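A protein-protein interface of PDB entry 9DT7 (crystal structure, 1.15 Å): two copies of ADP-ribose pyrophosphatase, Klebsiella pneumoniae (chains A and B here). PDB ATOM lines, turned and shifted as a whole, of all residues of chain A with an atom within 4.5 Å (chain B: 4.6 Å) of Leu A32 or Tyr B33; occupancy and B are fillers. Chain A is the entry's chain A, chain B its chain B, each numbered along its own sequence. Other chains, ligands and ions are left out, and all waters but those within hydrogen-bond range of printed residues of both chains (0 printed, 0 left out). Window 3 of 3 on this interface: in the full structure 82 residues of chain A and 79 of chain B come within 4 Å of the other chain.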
ATOM      1  N   GLU A  30      28.430  34.541   2.938  1.00  0.00           N
ATOM      2  CA  GLU A  30      27.148  34.313   3.590  1.00  0.00           C
ATOM      3  C   GLU A  30      27.068  32.848   3.988  1.00  0.00           C
ATOM      4  O   GLU A  30      27.544  31.989   3.256  1.00  0.00           O
ATOM      5  CB  GLU A  30      26.016  34.706   2.608  1.00  0.00           C
ATOM      6  CG  GLU A  30      24.615  34.544   3.133  1.00  0.00           C
ATOM      7  CD  GLU A  30      23.538  35.260   2.312  1.00  0.00           C
ATOM      8  OE1 GLU A  30      23.855  35.988   1.340  1.00  0.00           O
ATOM      9  OE2 GLU A  30      22.359  35.102   2.693  1.00  0.00           O
ATOM     10  N   THR A  31      26.468  32.565   5.154  1.00  0.00           N
ATOM     11  CA  THR A  31      26.154  31.195   5.554  1.00  0.00           C
ATOM     12  C   THR A  31      24.702  30.946   5.195  1.00  0.00           C
ATOM     13  O   THR A  31      23.802  31.580   5.746  1.00  0.00           O
ATOM     14  CB  THR A  31      26.445  30.934   7.031  1.00  0.00           C
ATOM     15  OG1 THR A  31      27.854  31.032   7.221  1.00  0.00           O
ATOM     16  CG2 THR A  31      25.975  29.535   7.449  1.00  0.00           C
ATOM     17  N   LEU A  32      24.490  30.040   4.243  1.00  0.00           N
ATOM     18  CA  LEU A  32      23.166  29.715   3.743  1.00  0.00           C
ATOM     19  C   LEU A  32      22.510  28.584   4.512  1.00  0.00           C
ATOM     20  O   LEU A  32      21.282  28.465   4.457  1.00  0.00           O
ATOM     21  CB  LEU A  32      23.215  29.312   2.271  1.00  0.00           C
ATOM     22  CG  LEU A  32      23.719  30.414   1.323  1.00  0.00           C
ATOM     23  CD1 LEU A  32      23.755  29.928  -0.111  1.00  0.00           C
ATOM     24  CD2 LEU A  32      22.870  31.671   1.390  1.00  0.00           C
ATOM     25  N   TYR A  33      23.288  27.730   5.181  1.00  0.00           N
ATOM     26  CA  TYR A  33      22.757  26.643   5.989  1.00  0.00           C
ATOM     27  C   TYR A  33      23.709  26.469   7.150  1.00  0.00           C
ATOM     28  O   TYR A  33      24.932  26.429   6.946  1.00  0.00           O
ATOM     29  CB  TYR A  33      22.663  25.300   5.227  1.00  0.00           C
ATOM     30  CG  TYR A  33      22.328  24.166   6.192  1.00  0.00           C
ATOM     31  CD1 TYR A  33      21.021  23.903   6.551  1.00  0.00           C
ATOM     32  CD2 TYR A  33      23.328  23.389   6.801  1.00  0.00           C
ATOM     33  CE1 TYR A  33      20.717  22.914   7.486  1.00  0.00           C
ATOM     34  CE2 TYR A  33      23.020  22.399   7.727  1.00  0.00           C
ATOM     35  CZ  TYR A  33      21.722  22.179   8.067  1.00  0.00           C
ATOM     36  OH  TYR A  33      21.378  21.207   8.983  1.00  0.00           O
ATOM     37  N   ARG A  34      23.164  26.379   8.354  1.00  0.00           N
ATOM     38  CA  ARG A  34      23.981  26.096   9.519  1.00  0.00           C
ATOM     39  C   ARG A  34      23.301  25.022  10.356  1.00  0.00           C
ATOM     40  O   ARG A  34      22.178  25.220  10.831  1.00  0.00           O
ATOM     41  CB  ARG A  34      24.181  27.365  10.349  1.00  0.00           C
ATOM     42  CG  ARG A  34      25.186  27.212  11.467  1.00  0.00           C
ATOM     43  CD  ARG A  34      26.536  27.451  10.831  1.00  0.00           C
ATOM     44  NE  ARG A  34      27.718  27.275  11.660  1.00  0.00           N
ATOM     45  CZ  ARG A  34      28.928  27.757  11.369  1.00  0.00           C
ATOM     46  NH1 ARG A  34      29.181  28.375  10.209  1.00  0.00           N
ATOM     47  NH2 ARG A  34      29.896  27.658  12.270  1.00  0.00           N
ATOM     48  N   LEU A  39      27.017  25.452   5.082  1.00  0.00           N
ATOM     49  CA  LEU A  39      27.119  25.635   3.633  1.00  0.00           C
ATOM     50  C   LEU A  39      27.211  27.141   3.429  1.00  0.00           C
ATOM     51  O   LEU A  39      26.263  27.878   3.730  1.00  0.00           O
ATOM     52  CB  LEU A  39      25.928  25.031   2.886  1.00  0.00           C
ATOM     53  CG  LEU A  39      26.068  24.832   1.371  1.00  0.00           C
ATOM     54  CD1 LEU A  39      26.034  26.167   0.673  1.00  0.00           C
ATOM     55  CD2 LEU A  39      27.315  24.030   0.975  1.00  0.00           C
ATOM     56  N   LEU A  41      28.465  30.663   1.058  1.00  0.00           N
ATOM     57  CA  LEU A  41      28.554  31.210  -0.291  1.00  0.00           C
ATOM     58  C   LEU A  41      29.597  32.311  -0.278  1.00  0.00           C
ATOM     59  O   LEU A  41      29.465  33.261   0.490  1.00  0.00           O
ATOM     60  CB  LEU A  41      27.183  31.754  -0.699  1.00  0.00           C
ATOM     61  CG  LEU A  41      27.012  32.163  -2.153  1.00  0.00           C
ATOM     62  CD1 LEU A  41      26.866  30.938  -3.018  1.00  0.00           C
ATOM     63  CD2 LEU A  41      25.818  33.102  -2.319  1.00  0.00           C
ATOM     64  N   GLU A  60      29.664  28.008  -3.830  1.00  0.00           N
ATOM     65  CA  GLU A  60      29.218  27.338  -2.612  1.00  0.00           C
ATOM     66  C   GLU A  60      30.379  26.549  -2.033  1.00  0.00           C
ATOM     67  O   GLU A  60      31.132  25.918  -2.775  1.00  0.00           O
ATOM     68  CB  GLU A  60      28.068  26.380  -2.915  1.00  0.00           C
ATOM     69  CG  GLU A  60      26.805  27.069  -3.355  1.00  0.00           C
ATOM     70  CD  GLU A  60      25.694  26.118  -3.740  1.00  0.00           C
ATOM     71  OE1 GLU A  60      25.892  24.913  -3.615  1.00  0.00           O
ATOM     72  OE2 GLU A  60      24.608  26.575  -4.161  1.00  0.00           O
ATOM     73  N   THR B  31      16.578  16.686   2.084  1.00  0.00           N
ATOM     74  CA  THR B  31      17.434  17.752   1.573  1.00  0.00           C
ATOM     75  C   THR B  31      17.384  18.922   2.547  1.00  0.00           C
ATOM     76  O   THR B  31      16.315  19.487   2.795  1.00  0.00           O
ATOM     77  CB  THR B  31      16.963  18.144   0.174  1.00  0.00           C
ATOM     78  OG1 THR B  31      17.126  16.993  -0.673  1.00  0.00           O
ATOM     79  CG2 THR B  31      17.761  19.320  -0.372  1.00  0.00           C
ATOM     80  N   LEU B  32      18.524  19.307   3.082  1.00  0.00           N
ATOM     81  CA  LEU B  32      18.681  20.427   3.996  1.00  0.00           C
ATOM     82  C   LEU B  32      18.982  21.722   3.255  1.00  0.00           C
ATOM     83  O   LEU B  32      18.562  22.798   3.673  1.00  0.00           O
ATOM     84  CB  LEU B  32      19.845  20.118   4.942  1.00  0.00           C
ATOM     85  CG  LEU B  32      19.655  18.928   5.880  1.00  0.00           C
ATOM     86  CD1 LEU B  32      20.972  18.627   6.609  1.00  0.00           C
ATOM     87  CD2 LEU B  32      18.560  19.165   6.862  1.00  0.00           C
ATOM     88  N   TYR B  33      19.750  21.628   2.178  1.00  0.00           N
ATOM     89  CA  TYR B  33      20.120  22.750   1.331  1.00  0.00           C
ATOM     90  C   TYR B  33      20.143  22.249  -0.103  1.00  0.00           C
ATOM     91  O   TYR B  33      20.779  21.237  -0.392  1.00  0.00           O
ATOM     92  CB  TYR B  33      21.509  23.319   1.693  1.00  0.00           C
ATOM     93  CG  TYR B  33      21.957  24.372   0.670  1.00  0.00           C
ATOM     94  CD1 TYR B  33      21.470  25.661   0.747  1.00  0.00           C
ATOM     95  CD2 TYR B  33      22.799  24.051  -0.411  1.00  0.00           C
ATOM     96  CE1 TYR B  33      21.811  26.610  -0.202  1.00  0.00           C
ATOM     97  CE2 TYR B  33      23.166  24.992  -1.366  1.00  0.00           C
ATOM     98  CZ  TYR B  33      22.659  26.276  -1.256  1.00  0.00           C
ATOM     99  OH  TYR B  33      22.986  27.255  -2.178  1.00  0.00           O
ATOM    100  N   ARG B  34      19.461  22.960  -0.996  1.00  0.00           N
ATOM    101  CA  ARG B  34      19.341  22.597  -2.409  1.00  0.00           C
ATOM    102  C   ARG B  34      19.874  23.762  -3.229  1.00  0.00           C
ATOM    103  O   ARG B  34      19.201  24.785  -3.348  1.00  0.00           O
ATOM    104  CB  ARG B  34      17.875  22.337  -2.777  1.00  0.00           C
ATOM    105  CG  ARG B  34      17.643  21.702  -4.165  1.00  0.00           C
ATOM    106  CD  ARG B  34      16.145  21.632  -4.562  1.00  0.00           C
ATOM    107  NE  ARG B  34      15.324  20.947  -3.570  1.00  0.00           N
ATOM    108  CZ  ARG B  34      15.287  19.635  -3.426  1.00  0.00           C
ATOM    109  NH1 ARG B  34      15.982  18.838  -4.220  1.00  0.00           N
ATOM    110  NH2 ARG B  34      14.548  19.108  -2.454  1.00  0.00           N
ATOM    111  N   GLY B  35      21.044  23.629  -3.810  1.00  0.00           N
ATOM    112  CA  GLY B  35      21.629  24.695  -4.614  1.00  0.00           C
ATOM    113  C   GLY B  35      22.401  24.118  -5.756  1.00  0.00           C
ATOM    114  O   GLY B  35      21.992  23.112  -6.350  1.00  0.00           O
ATOM    115  N   PHE B  37      25.277  22.660  -5.314  1.00  0.00           N
ATOM    116  CA  PHE B  37      25.503  21.427  -4.588  1.00  0.00           C
ATOM    117  C   PHE B  37      24.329  21.261  -3.626  1.00  0.00           C
ATOM    118  O   PHE B  37      23.458  22.135  -3.525  1.00  0.00           O
ATOM    119  CB  PHE B  37      26.768  21.558  -3.774  1.00  0.00           C
ATOM    120  CG  PHE B  37      28.008  21.830  -4.570  1.00  0.00           C
ATOM    121  CD1 PHE B  37      28.304  21.118  -5.728  1.00  0.00           C
ATOM    122  CD2 PHE B  37      28.922  22.771  -4.118  1.00  0.00           C
ATOM    123  CE1 PHE B  37      29.485  21.367  -6.435  1.00  0.00           C
ATOM    124  CE2 PHE B  37      30.108  23.013  -4.804  1.00  0.00           C
ATOM    125  CZ  PHE B  37      30.390  22.297  -5.947  1.00  0.00           C
ATOM    126  N   SER B  38      24.299  20.162  -2.892  1.00  0.00           N
ATOM    127  CA  SER B  38      23.268  19.930  -1.894  1.00  0.00           C
ATOM    128  C   SER B  38      23.893  19.465  -0.590  1.00  0.00           C
ATOM    129  O   SER B  38      24.993  18.909  -0.555  1.00  0.00           O
ATOM    130  CB  SER B  38      22.249  18.907  -2.393  1.00  0.00           C
ATOM    131  OG  SER B  38      21.474  19.463  -3.440  1.00  0.00           O
ATOM    132  N   LEU B  39      23.130  19.652   0.477  1.00  0.00           N
ATOM    133  CA  LEU B  39      23.438  19.055   1.767  1.00  0.00           C
ATOM    134  C   LEU B  39      22.219  18.242   2.173  1.00  0.00           C
ATOM    135  O   LEU B  39      21.118  18.777   2.211  1.00  0.00           O
ATOM    136  CB  LEU B  39      23.722  20.127   2.796  1.00  0.00           C
ATOM    137  CG  LEU B  39      24.274  19.600   4.102  1.00  0.00           C
ATOM    138  CD1 LEU B  39      25.703  19.095   3.979  1.00  0.00           C
ATOM    139  CD2 LEU B  39      24.182  20.659   5.143  1.00  0.00           C
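OE2 of Glu A60 is in hydrogen-bond range of OH of Tyr B33 (2.7 Å).
OE1 of Glu A60 lies within hydrogen-bond range of N of Phe B37 (2.9 Å).
N of Leu A39 lies within hydrogen-bond range of O of Tyr A33.
O of Tyr B33 lies within hydrogen-bond range of N of Leu B39 (3.0 Å).
O of Leu A39 lies within hydrogen-bond range of N of Leu A32, 2.8 Å away.
N of Leu B32 sits at hydrogen-bond distance from O of Leu B39 (2.8 Å).
Among the printed residues, pairs that only touch across the chains: Tyr A33 with Leu B39 (3.3 Å), Leu A32 with Tyr B33 (3.5 Å), Tyr A33 with Leu B32 (3.5 Å), Glu A60 with Gly B35 (3.6 Å) and Leu A39 with Tyr B33 (3.7 Å).
Leu A32 touches just one residue of chain B: Tyr B33.
Of the printed residues of chain B, Tyr A33 touches Leu B32 (3.5 Å) and Leu B39 (3.3 Å).
Arg B34 touches none of the printed residues of chain A.
Printed residues of chain A within 4 Å of Phe B37: Glu A60.
Ser B38 touches none of the printed residues of chain A.
The nearest printed residue of chain B that does not touch Leu A32 is Leu B32 (6.3 Å).
The nearest printed residue of chain B that does not touch Tyr A33 is Tyr B33 (4.2 Å).
Of the 8 printed residues of chain B, 5 touch a printed residue of chain A.
Printed residues of chain B that touch a printed residue of chain A: Leu B32, Tyr B33, Gly B35, Phe B37 and Leu B39.
Among the printed residues, no Asp or Glu carboxylate lies within 4 Å of a Lys or Arg side-chain nitrogen of the other chain.
Leu A32 touches Tyr B33, and with the chains exchanged Tyr A33 touches Leu B32.
Tyr A33 touches Leu B39, and with the chains exchanged Leu A39 touches Tyr B33.
Of the 7 pairs that touch across the chains among the printed residues, 4 have their exchanged pair printed and touching as well.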
